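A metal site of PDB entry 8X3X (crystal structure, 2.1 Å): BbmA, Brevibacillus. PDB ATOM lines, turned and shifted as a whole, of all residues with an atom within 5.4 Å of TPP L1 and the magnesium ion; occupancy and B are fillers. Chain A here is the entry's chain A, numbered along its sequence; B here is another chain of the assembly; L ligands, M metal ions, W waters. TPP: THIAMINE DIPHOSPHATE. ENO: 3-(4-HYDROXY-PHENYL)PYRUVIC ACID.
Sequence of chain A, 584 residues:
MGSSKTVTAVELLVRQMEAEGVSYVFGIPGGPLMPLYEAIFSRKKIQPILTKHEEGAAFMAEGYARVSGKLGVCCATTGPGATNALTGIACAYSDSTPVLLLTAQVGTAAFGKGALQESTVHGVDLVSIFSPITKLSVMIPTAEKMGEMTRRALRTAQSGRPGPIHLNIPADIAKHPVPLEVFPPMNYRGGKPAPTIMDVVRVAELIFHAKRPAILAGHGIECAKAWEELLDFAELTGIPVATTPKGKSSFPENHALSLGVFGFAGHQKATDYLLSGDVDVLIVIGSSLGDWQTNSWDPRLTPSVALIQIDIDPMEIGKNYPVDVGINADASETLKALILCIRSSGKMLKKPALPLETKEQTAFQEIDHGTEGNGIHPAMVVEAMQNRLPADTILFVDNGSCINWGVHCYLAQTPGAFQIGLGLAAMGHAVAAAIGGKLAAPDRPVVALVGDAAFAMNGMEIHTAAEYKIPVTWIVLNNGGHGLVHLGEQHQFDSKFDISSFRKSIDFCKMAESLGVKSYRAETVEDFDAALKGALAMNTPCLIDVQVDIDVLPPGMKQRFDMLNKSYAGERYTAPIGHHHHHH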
ATOM      1  N   ASN A 399     -26.419  13.413   6.875  1.00  0.00           N
ATOM      2  CA  ASN A 399     -25.518  14.015   5.920  1.00  0.00           C
ATOM      3  C   ASN A 399     -24.274  13.146   5.832  1.00  0.00           C
ATOM      4  O   ASN A 399     -23.683  12.797   6.861  1.00  0.00           O
ATOM      5  CB  ASN A 399     -25.223  15.461   6.340  1.00  0.00           C
ATOM      6  CG  ASN A 399     -26.509  16.319   6.382  1.00  0.00           C
ATOM      7  OD1 ASN A 399     -27.101  16.624   5.338  1.00  0.00           O
ATOM      8  ND2 ASN A 399     -26.945  16.693   7.599  1.00  0.00           N
ATOM      9  N   GLY A 400     -23.890  12.793   4.624  1.00  0.00           N
ATOM     10  CA  GLY A 400     -23.048  11.660   4.295  1.00  0.00           C
ATOM     11  C   GLY A 400     -23.633  11.009   3.066  1.00  0.00           C
ATOM     12  O   GLY A 400     -24.549  11.545   2.435  1.00  0.00           O
ATOM     13  N   SER A 401     -23.121   9.813   2.718  1.00  0.00           N
ATOM     14  CA  SER A 401     -23.653   9.104   1.564  1.00  0.00           C
ATOM     15  C   SER A 401     -25.145   8.831   1.694  1.00  0.00           C
ATOM     16  O   SER A 401     -25.804   8.570   0.683  1.00  0.00           O
ATOM     17  CB  SER A 401     -22.913   7.780   1.352  1.00  0.00           C
ATOM     18  OG  SER A 401     -23.355   6.800   2.281  1.00  0.00           O
ATOM     19  N   CYS A 402     -25.690   8.870   2.913  1.00  0.00           N
ATOM     20  CA  CYS A 402     -27.133   8.706   3.071  1.00  0.00           C
ATOM     21  C   CYS A 402     -27.916   9.790   2.333  1.00  0.00           C
ATOM     22  O   CYS A 402     -29.048   9.551   1.899  1.00  0.00           O
ATOM     23  CB  CYS A 402     -27.490   8.676   4.554  1.00  0.00           C
ATOM     24  SG  CYS A 402     -27.041  10.172   5.431  1.00  0.00           S
ATOM     25  N   LEU A 424     -27.042  23.505   5.852  1.00  0.00           N
ATOM     26  CA  LEU A 424     -25.692  23.371   6.384  1.00  0.00           C
ATOM     27  C   LEU A 424     -25.169  21.953   6.284  1.00  0.00           C
ATOM     28  O   LEU A 424     -23.952  21.748   6.364  1.00  0.00           O
ATOM     29  CB  LEU A 424     -25.655  23.820   7.854  1.00  0.00           C
ATOM     30  CG  LEU A 424     -24.384  24.460   8.412  1.00  0.00           C
ATOM     31  CD1 LEU A 424     -23.839  25.549   7.493  1.00  0.00           C
ATOM     32  CD2 LEU A 424     -24.674  25.017   9.781  1.00  0.00           C
ATOM     33  N   ALA A 425     -26.048  20.970   6.107  1.00  0.00           N
ATOM     34  CA  ALA A 425     -25.659  19.566   5.938  1.00  0.00           C
ATOM     35  C   ALA A 425     -24.713  19.130   7.059  1.00  0.00           C
ATOM     36  O   ALA A 425     -23.623  18.596   6.822  1.00  0.00           O
ATOM     37  CB  ALA A 425     -25.036  19.325   4.558  1.00  0.00           C
ATOM     38  N   ALA A 426     -25.135  19.356   8.286  1.00  0.00           N
ATOM     39  CA  ALA A 426     -24.318  19.020   9.442  1.00  0.00           C
ATOM     40  C   ALA A 426     -24.472  17.552   9.760  1.00  0.00           C
ATOM     41  O   ALA A 426     -25.595  17.051   9.910  1.00  0.00           O
ATOM     42  CB  ALA A 426     -24.722  19.882  10.636  1.00  0.00           C
ATOM     43  N   MET A 427     -23.345  16.845   9.864  1.00  0.00           N
ATOM     44  CA  MET A 427     -23.387  15.460  10.321  1.00  0.00           C
ATOM     45  C   MET A 427     -24.039  15.395  11.681  1.00  0.00           C
ATOM     46  O   MET A 427     -23.768  16.221  12.551  1.00  0.00           O
ATOM     47  CB  MET A 427     -21.983  14.883  10.409  1.00  0.00           C
ATOM     48  CG  MET A 427     -21.418  14.488   9.087  1.00  0.00           C
ATOM     49  SD  MET A 427     -19.703  14.040   9.324  1.00  0.00           S
ATOM     50  CE  MET A 427     -19.831  12.670  10.488  1.00  0.00           C
ATOM     51  N   GLY A 451     -25.479   7.799   8.740  1.00  0.00           N
ATOM     52  CA  GLY A 451     -24.198   7.109   8.669  1.00  0.00           C
ATOM     53  C   GLY A 451     -23.590   6.836  10.052  1.00  0.00           C
ATOM     54  O   GLY A 451     -24.049   7.365  11.067  1.00  0.00           O
ATOM     55  N   ASP A 452     -22.542   6.014  10.061  1.00  0.00           N
ATOM     56  CA  ASP A 452     -21.949   5.599  11.340  1.00  0.00           C
ATOM     57  C   ASP A 452     -21.141   6.720  11.980  1.00  0.00           C
ATOM     58  O   ASP A 452     -21.172   6.874  13.212  1.00  0.00           O
ATOM     59  CB  ASP A 452     -21.094   4.342  11.164  1.00  0.00           C
ATOM     60  CG  ASP A 452     -19.969   4.487  10.121  1.00  0.00           C
ATOM     61  OD1 ASP A 452     -20.240   4.866   8.968  1.00  0.00           O
ATOM     62  OD2 ASP A 452     -18.818   4.181  10.471  1.00  0.00           O
ATOM     63  N   ALA A 453     -20.413   7.501  11.176  1.00  0.00           N
ATOM     64  CA  ALA A 453     -19.656   8.611  11.764  1.00  0.00           C
ATOM     65  C   ALA A 453     -20.593   9.681  12.312  1.00  0.00           C
ATOM     66  O   ALA A 453     -20.325  10.266  13.375  1.00  0.00           O
ATOM     67  CB  ALA A 453     -18.699   9.216  10.751  1.00  0.00           C
ATOM     68  N   ALA A 454     -21.676   9.961  11.596  1.00  0.00           N
ATOM     69  CA  ALA A 454     -22.682  10.886  12.115  1.00  0.00           C
ATOM     70  C   ALA A 454     -23.263  10.379  13.431  1.00  0.00           C
ATOM     71  O   ALA A 454     -23.502  11.174  14.357  1.00  0.00           O
ATOM     72  CB  ALA A 454     -23.794  11.093  11.087  1.00  0.00           C
ATOM     73  N   PHE A 455     -23.499   9.064  13.531  1.00  0.00           N
ATOM     74  CA  PHE A 455     -24.052   8.516  14.759  1.00  0.00           C
ATOM     75  C   PHE A 455     -23.041   8.592  15.899  1.00  0.00           C
ATOM     76  O   PHE A 455     -23.414   8.856  17.054  1.00  0.00           O
ATOM     77  CB  PHE A 455     -24.525   7.076  14.556  1.00  0.00           C
ATOM     78  CG  PHE A 455     -25.495   6.615  15.601  1.00  0.00           C
ATOM     79  CD1 PHE A 455     -26.855   6.848  15.447  1.00  0.00           C
ATOM     80  CD2 PHE A 455     -25.055   5.961  16.745  1.00  0.00           C
ATOM     81  CE1 PHE A 455     -27.753   6.453  16.415  1.00  0.00           C
ATOM     82  CE2 PHE A 455     -25.955   5.545  17.720  1.00  0.00           C
ATOM     83  CZ  PHE A 455     -27.314   5.797  17.541  1.00  0.00           C
ATOM     84  N   MET A 457     -21.282  10.999  16.291  1.00  0.00           N
ATOM     85  CA  MET A 457     -21.240  12.409  16.652  1.00  0.00           C
ATOM     86  C   MET A 457     -22.384  12.816  17.574  1.00  0.00           C
ATOM     87  O   MET A 457     -22.173  13.603  18.494  1.00  0.00           O
ATOM     88  CB  MET A 457     -21.252  13.258  15.379  1.00  0.00           C
ATOM     89  CG  MET A 457     -20.278  14.399  15.371  1.00  0.00           C
ATOM     90  SD  MET A 457     -20.309  15.223  13.764  1.00  0.00           S
ATOM     91  CE  MET A 457     -18.903  14.507  12.920  1.00  0.00           C
ATOM     92  N   LEU A 477     -26.167   3.154   8.578  1.00  0.00           N
ATOM     93  CA  LEU A 477     -25.420   2.552   7.486  1.00  0.00           C
ATOM     94  C   LEU A 477     -23.972   2.456   7.940  1.00  0.00           C
ATOM     95  O   LEU A 477     -23.197   3.416   7.833  1.00  0.00           O
ATOM     96  CB  LEU A 477     -25.543   3.364   6.209  1.00  0.00           C
ATOM     97  CG  LEU A 477     -26.924   3.559   5.542  1.00  0.00           C
ATOM     98  CD1 LEU A 477     -26.754   4.450   4.328  1.00  0.00           C
ATOM     99  CD2 LEU A 477     -27.600   2.243   5.136  1.00  0.00           C
ATOM    100  N   ASN A 479     -20.539   1.564   7.507  1.00  0.00           N
ATOM    101  CA  ASN A 479     -19.491   1.176   6.570  1.00  0.00           C
ATOM    102  C   ASN A 479     -18.092   1.351   7.149  1.00  0.00           C
ATOM    103  O   ASN A 479     -17.112   1.338   6.401  1.00  0.00           O
ATOM    104  CB  ASN A 479     -19.643   1.942   5.248  1.00  0.00           C
ATOM    105  CG  ASN A 479     -19.665   3.430   5.430  1.00  0.00           C
ATOM    106  OD1 ASN A 479     -19.322   3.945   6.490  1.00  0.00           O
ATOM    107  ND2 ASN A 479     -20.056   4.148   4.375  1.00  0.00           N
ATOM    108  N   GLY A 480     -17.987   1.520   8.464  1.00  0.00           N
ATOM    109  CA  GLY A 480     -16.689   1.566   9.134  1.00  0.00           C
ATOM    110  C   GLY A 480     -15.886   2.811   8.845  1.00  0.00           C
ATOM    111  O   GLY A 480     -14.665   2.719   8.619  1.00  0.00           O
ATOM    112  N   GLY A 481     -16.528   3.977   8.814  1.00  0.00           N
ATOM    113  CA  GLY A 481     -15.800   5.216   8.662  1.00  0.00           C
ATOM    114  C   GLY A 481     -16.547   6.205   7.787  1.00  0.00           C
ATOM    115  O   GLY A 481     -17.769   6.150   7.640  1.00  0.00           O
ATOM    116  N   HIS A 482     -15.782   7.139   7.229  1.00  0.00           N
ATOM    117  CA  HIS A 482     -16.306   8.266   6.455  1.00  0.00           C
ATOM    118  C   HIS A 482     -16.327   7.889   4.989  1.00  0.00           C
ATOM    119  O   HIS A 482     -15.355   8.103   4.254  1.00  0.00           O
ATOM    120  CB  HIS A 482     -15.461   9.509   6.709  1.00  0.00           C
ATOM    121  CG  HIS A 482     -15.411   9.927   8.140  1.00  0.00           C
ATOM    122  ND1 HIS A 482     -15.957  11.109   8.592  1.00  0.00           N
ATOM    123  CD2 HIS A 482     -14.877   9.327   9.235  1.00  0.00           C
ATOM    124  CE1 HIS A 482     -15.747  11.221   9.889  1.00  0.00           C
ATOM    125  NE2 HIS A 482     -15.097  10.155  10.308  1.00  0.00           N
ATOM    126  N   GLY A 483     -17.464   7.357   4.531  1.00  0.00           N
ATOM    127  CA  GLY A 483     -17.547   6.831   3.171  1.00  0.00           C
ATOM    128  C   GLY A 483     -17.291   7.898   2.115  1.00  0.00           C
ATOM    129  O   GLY A 483     -16.466   7.701   1.211  1.00  0.00           O
ATOM    130  N   LEU A 484     -17.993   9.031   2.214  1.00  0.00           N
ATOM    131  CA  LEU A 484     -17.792  10.080   1.218  1.00  0.00           C
ATOM    132  C   LEU A 484     -16.343  10.529   1.166  1.00  0.00           C
ATOM    133  O   LEU A 484     -15.791  10.747   0.073  1.00  0.00           O
ATOM    134  CB  LEU A 484     -18.717  11.259   1.506  1.00  0.00           C
ATOM    135  CG  LEU A 484     -20.220  11.036   1.262  1.00  0.00           C
ATOM    136  CD1 LEU A 484     -20.945  12.394   1.155  1.00  0.00           C
ATOM    137  CD2 LEU A 484     -20.480  10.183   0.026  1.00  0.00           C
ATOM    138  N   VAL A 485     -15.689  10.679   2.320  1.00  0.00           N
ATOM    139  CA  VAL A 485     -14.279  11.096   2.321  1.00  0.00           C
ATOM    140  C   VAL A 485     -13.414  10.020   1.700  1.00  0.00           C
ATOM    141  O   VAL A 485     -12.506  10.314   0.907  1.00  0.00           O
ATOM    142  CB  VAL A 485     -13.798  11.427   3.748  1.00  0.00           C
ATOM    143  CG1 VAL A 485     -12.315  11.876   3.698  1.00  0.00           C
ATOM    144  CG2 VAL A 485     -14.667  12.477   4.401  1.00  0.00           C
ATOM    145  N   ILE B  28     -11.492  16.593  11.763  1.00  0.00           N
ATOM    146  CA  ILE B  28     -12.331  15.740  10.926  1.00  0.00           C
ATOM    147  C   ILE B  28     -12.278  16.332   9.519  1.00  0.00           C
ATOM    148  O   ILE B  28     -12.530  17.542   9.339  1.00  0.00           O
ATOM    149  CB  ILE B  28     -13.778  15.674  11.449  1.00  0.00           C
ATOM    150  CG1 ILE B  28     -13.822  15.068  12.862  1.00  0.00           C
ATOM    151  CG2 ILE B  28     -14.670  14.883  10.496  1.00  0.00           C
ATOM    152  CD1 ILE B  28     -15.158  15.231  13.595  1.00  0.00           C
ATOM    153  N   PRO B  29     -11.966  15.546   8.503  1.00  0.00           N
ATOM    154  CA  PRO B  29     -11.849  16.100   7.151  1.00  0.00           C
ATOM    155  C   PRO B  29     -13.184  16.551   6.583  1.00  0.00           C
ATOM    156  O   PRO B  29     -14.268  16.277   7.113  1.00  0.00           O
ATOM    157  CB  PRO B  29     -11.271  14.928   6.335  1.00  0.00           C
ATOM    158  CG  PRO B  29     -11.798  13.720   7.068  1.00  0.00           C
ATOM    159  CD  PRO B  29     -11.695  14.098   8.531  1.00  0.00           C
ATOM    160  N   GLY B  30     -13.075  17.279   5.475  1.00  0.00           N
ATOM    161  CA  GLY B  30     -14.208  17.685   4.649  1.00  0.00           C
ATOM    162  C   GLY B  30     -13.664  18.061   3.289  1.00  0.00           C
ATOM    163  O   GLY B  30     -12.474  18.350   3.142  1.00  0.00           O
ATOM    164  N   GLU B  54     -15.794  17.473  16.137  1.00  0.00           N
ATOM    165  CA  GLU B  54     -14.797  18.546  16.074  1.00  0.00           C
ATOM    166  C   GLU B  54     -14.647  19.249  17.420  1.00  0.00           C
ATOM    167  O   GLU B  54     -13.604  19.851  17.690  1.00  0.00           O
ATOM    168  CB  GLU B  54     -15.155  19.567  14.993  1.00  0.00           C
ATOM    169  CG  GLU B  54     -15.015  19.021  13.605  1.00  0.00           C
ATOM    170  CD  GLU B  54     -16.319  18.418  13.082  1.00  0.00           C
ATOM    171  OE1 GLU B  54     -16.406  18.214  11.861  1.00  0.00           O
ATOM    172  OE2 GLU B  54     -17.234  18.139  13.886  1.00  0.00           O
ATOM    173  N   THR B  77     -13.892  21.452   8.665  1.00  0.00           N
ATOM    174  CA  THR B  77     -14.374  21.838   7.353  1.00  0.00           C
ATOM    175  C   THR B  77     -15.274  23.067   7.449  1.00  0.00           C
ATOM    176  O   THR B  77     -15.477  23.653   8.515  1.00  0.00           O
ATOM    177  CB  THR B  77     -15.115  20.680   6.680  1.00  0.00           C
ATOM    178  OG1 THR B  77     -15.284  20.979   5.290  1.00  0.00           O
ATOM    179  CG2 THR B  77     -16.493  20.433   7.344  1.00  0.00           C
ATOM    180  N   PRO B  80     -20.670  23.534   9.407  1.00  0.00           N
ATOM    181  CA  PRO B  80     -20.924  22.845  10.690  1.00  0.00           C
ATOM    182  C   PRO B  80     -19.689  22.175  11.275  1.00  0.00           C
ATOM    183  O   PRO B  80     -19.645  21.946  12.492  1.00  0.00           O
ATOM    184  CB  PRO B  80     -21.992  21.811  10.321  1.00  0.00           C
ATOM    185  CG  PRO B  80     -21.670  21.461   8.876  1.00  0.00           C
ATOM    186  CD  PRO B  80     -21.201  22.783   8.256  1.00  0.00           C
ATOM    187  N   GLY B  81     -18.692  21.824  10.468  1.00  0.00           N
ATOM    188  CA  GLY B  81     -17.447  21.344  11.037  1.00  0.00           C
ATOM    189  C   GLY B  81     -16.852  22.372  11.986  1.00  0.00           C
ATOM    190  O   GLY B  81     -16.587  22.079  13.162  1.00  0.00           O
ATOM    191  N   ASN B  84     -18.933  23.236  15.156  1.00  0.00           N
ATOM    192  CA  ASN B  84     -18.821  22.176  16.149  1.00  0.00           C
ATOM    193  C   ASN B  84     -17.606  22.352  17.056  1.00  0.00           C
ATOM    194  O   ASN B  84     -17.596  21.846  18.176  1.00  0.00           O
ATOM    195  CB  ASN B  84     -18.721  20.794  15.468  1.00  0.00           C
ATOM    196  CG  ASN B  84     -20.088  20.112  15.313  1.00  0.00           C
ATOM    197  OD1 ASN B  84     -21.110  20.651  15.695  1.00  0.00           O
ATOM    198  ND2 ASN B  84     -20.087  18.901  14.752  1.00  0.00           N
ATOM    199  N   GLN B 117     -22.367  24.759   2.263  1.00  0.00           N
ATOM    200  CA  GLN B 117     -21.814  25.145   3.556  1.00  0.00           C
ATOM    201  C   GLN B 117     -21.075  26.482   3.477  1.00  0.00           C
ATOM    202  O   GLN B 117     -20.098  26.718   4.189  1.00  0.00           O
ATOM    203  CB  GLN B 117     -20.907  24.042   4.114  1.00  0.00           C
ATOM    204  CG  GLN B 117     -21.663  22.702   4.346  1.00  0.00           C
ATOM    205  CD  GLN B 117     -20.759  21.573   4.831  1.00  0.00           C
ATOM    206  OE1 GLN B 117     -19.559  21.601   4.609  1.00  0.00           O
ATOM    207  NE2 GLN B 117     -21.352  20.571   5.498  1.00  0.00           N
HETATM  208  N1' TPP L   1     -18.187  17.588  10.040  1.00  0.00           N
HETATM  209  C2' TPP L   1     -19.506  17.880  10.116  1.00  0.00           C
HETATM  210  CM2 TPP L   1     -20.036  18.262  11.459  1.00  0.00           C
HETATM  211  N3' TPP L   1     -20.373  17.858   9.103  1.00  0.00           N
HETATM  212  C4' TPP L   1     -19.907  17.506   7.893  1.00  0.00           C
HETATM  213  N4' TPP L   1     -20.786  17.504   6.879  1.00  0.00           N
HETATM  214  C5' TPP L   1     -18.530  17.184   7.696  1.00  0.00           C
HETATM  215  C6' TPP L   1     -17.742  17.242   8.826  1.00  0.00           C
HETATM  216  C7' TPP L   1     -17.962  16.782   6.369  1.00  0.00           C
HETATM  217  N3  TPP L   1     -18.479  15.478   5.904  1.00  0.00           N
HETATM  218  C2  TPP L   1     -19.420  15.342   4.994  1.00  0.00           C
HETATM  219  S1  TPP L   1     -19.806  13.735   4.713  1.00  0.00           S
HETATM  220  C5  TPP L   1     -18.641  13.220   5.880  1.00  0.00           C
HETATM  221  C4  TPP L   1     -18.032  14.270   6.454  1.00  0.00           C
HETATM  222  CM4 TPP L   1     -16.989  14.241   7.505  1.00  0.00           C
HETATM  223  C6  TPP L   1     -18.519  11.764   6.215  1.00  0.00           C
HETATM  224  C7  TPP L   1     -19.808  11.237   6.810  1.00  0.00           C
HETATM  225  O7  TPP L   1     -19.624   9.876   7.271  1.00  0.00           O
HETATM  226  PA  TPP L   1     -20.821   8.966   7.738  1.00  0.00           P
HETATM  227  O1A TPP L   1     -21.805   9.647   8.611  1.00  0.00           O
HETATM  228  O2A TPP L   1     -20.268   7.654   8.314  1.00  0.00           O
HETATM  229  O3A TPP L   1     -21.449   8.633   6.327  1.00  0.00           O
HETATM  230  PB  TPP L   1     -21.078   7.825   5.004  1.00  0.00           P
HETATM  231  O1B TPP L   1     -22.281   7.084   4.499  1.00  0.00           O
HETATM  232  O2B TPP L   1     -19.901   6.924   5.449  1.00  0.00           O
HETATM  233  O3B TPP L   1     -20.505   8.868   4.039  1.00  0.00           O
HETATM  234  O4  ENO L   2     -17.326  16.786   3.216  1.00  0.00           O
HETATM  235  C9  ENO L   2     -16.302  14.949  -0.450  1.00  0.00           C
HETATM  236  C8  ENO L   2     -15.113  14.883  -1.176  1.00  0.00           C
HETATM  237  C7  ENO L   2     -13.890  14.757  -0.520  1.00  0.00           C
HETATM  238  C6  ENO L   2     -13.846  14.682   0.866  1.00  0.00           C
HETATM  239  C5  ENO L   2     -15.030  14.726   1.587  1.00  0.00           C
HETATM  240  C4  ENO L   2     -16.245  14.853   0.937  1.00  0.00           C
HETATM  241  O3  ENO L   2     -12.690  14.698  -1.248  1.00  0.00           O
HETATM  242  C3  ENO L   2     -17.520  14.940   1.774  1.00  0.00           C
HETATM  243  C2  ENO L   2     -17.674  16.405   2.152  1.00  0.00           C
HETATM  244  C1  ENO L   2     -18.228  17.378   1.119  1.00  0.00           C
HETATM  245  O2  ENO L   2     -17.838  18.566   1.105  1.00  0.00           O
HETATM  246  O1  ENO L   2     -19.067  16.984   0.258  1.00  0.00           O
HETATM  247 MG    MG M   1     -19.817   5.935   7.324  1.00  0.00          MG
HETATM  248  O   HOH W   1     -24.406  10.200   7.836  1.00  0.00           O
HETATM  249  O   HOH W   2     -21.901   5.503   6.848  1.00  0.00           O
HETATM  250  O   HOH W   3     -24.616   8.267   5.506  1.00  0.00           O
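The backbone NH of Asp 452 lies close to an oxygen (O2A) of TPP L1, at 3.3 Å. N of Ser 401 lies within hydrogen-bond range of O3B of TPP L1, at 3.1 Å. An oxygen (O1B) of TPP L1 sits at hydrogen-bond distance from the side-chain hydroxyl (OG) of Ser 401. A nitrogen (N1') of TPP L1 lies within hydrogen-bond range of the side-chain carboxylate of Glu 54 of chain B (2.6 Å). The backbone NH of Gly 483 lies within hydrogen-bond range of an oxygen (O3B) of TPP L1, at 3.4 Å. The backbone NH of Ala 453 lies close to an oxygen (O2A) of TPP L1 (2.9 Å). N of Ala 454 sits at hydrogen-bond distance from O1A of TPP L1 (3.0 Å). The backbone carbonyl oxygen (O) of Ala 425 is in hydrogen-bond range of a nitrogen (N4') of TPP L1 (3.0 Å). N of Leu 484 is in hydrogen-bond range of O3B of TPP L1, at 3.1 Å. N of Met 427 lies within hydrogen-bond range of N3' of TPP L1, 3.2 Å away. The side-chain amide nitrogen of Gln 117 of chain B sits close to a nitrogen (N4') of TPP L1, 3.4 Å away.
N of Asp 452 is in hydrogen-bond range of O of Leu 477. The side-chain carboxylate (OD2) of Asp 452 sits at hydrogen-bond distance from the backbone NH (N) of Gly 480, at 3.4 Å. The side-chain carboxylate (OE2) of Glu 54 of chain B is in hydrogen-bond range of the side-chain amide nitrogen (ND2) of Asn 84 of chain B (3.1 Å). NE2 of Gln 117 of chain B is in hydrogen-bond range of O of Ala 425 (3.3 Å). NE2 of Gln 117 of chain B sits at hydrogen-bond distance from O of Leu 424 (3.0 Å).
CA of Gly 400 touches O3B of TPP L1, at 3.8 Å. CA of Gly 451 touches O1A of TPP L1, at 3.5 Å. SD of Met 457 touches CM2 of TPP L1 (3.8 Å). ND1 of His 482 touches CM4 of TPP L1, at 3.5 Å. CG2 of Ile 28 of chain B touches CM4 of TPP L1, at 3.8 Å. Pro 29 of chain B touches TPP L1 (O to CM4, 3.4 Å). Thr 77 of chain B touches TPP L1 (CG2 to C6', 3.7 Å). Pro 80 of chain B touches TPP L1. Gly 81 of chain B touches TPP L1 (N to CM2, 3.9 Å). ND2 of Asn 84 of chain B touches CM2 of TPP L1 (3.4 Å). Hydrophobic or aromatic side chains within 4 Å of TPP L1: Met 427, Ala 453, Ala 454, Met 457, His 482, Leu 484, Ile 28 of chain B and Pro 80 of chain B. Within 4 Å of TPP L1: Gly 400, Ser 401, Ala 425, Met 427, Gly 451, Asp 452, Ala 453, Ala 454, Met 457, Asn 479, Gly 481, His 482, Gly 483, Leu 484, Ile 28 of chain B, Pro 29 of chain B, Glu 54 of chain B, Thr 77 of chain B, Pro 80 of chain B, Gly 81 of chain B, Asn 84 of chain B and Gln 117 of chain B. The nearest printed residue that does not touch TPP L1 is Asn 399 (4.1 Å).
Merely in contact with the magnesium ion: Gly 483. Of the 31 residues printed, 4 come within 4 Å of the magnesium ion.
The magnesium ion is bound by OD1 of Asp 452 (2.0 Å), O2A of TPP L1 (2.0 Å), O of Gly 481 (2.1 Å), O2B of TPP L1 (2.1 Å), water W2 (2.2 Å) and OD1 of Asn 479 (2.2 Å). The magnesium ion has six donor atoms within binding distance.
Water W2 lies within hydrogen-bond range of the backbone carbonyl oxygen of Leu 477, an oxygen (O1B) of TPP L1, the backbone NH of Asp 452 and the side-chain amide nitrogen of Asn 479. Water W1 lies within hydrogen-bond range of an oxygen (O1A) of TPP L1 (2.8 Å), the backbone NH (N) of Gly 451 (2.8 Å), the backbone carbonyl oxygen (O) of Asn 399 (2.9 Å) and the side-chain sulfur (SG) of Cys 402 (3.6 Å). Water W3 lies within hydrogen-bond range of an oxygen (O1B) of TPP L1, the backbone NH (N) of Cys 402 and the backbone NH (N) of Gly 451.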
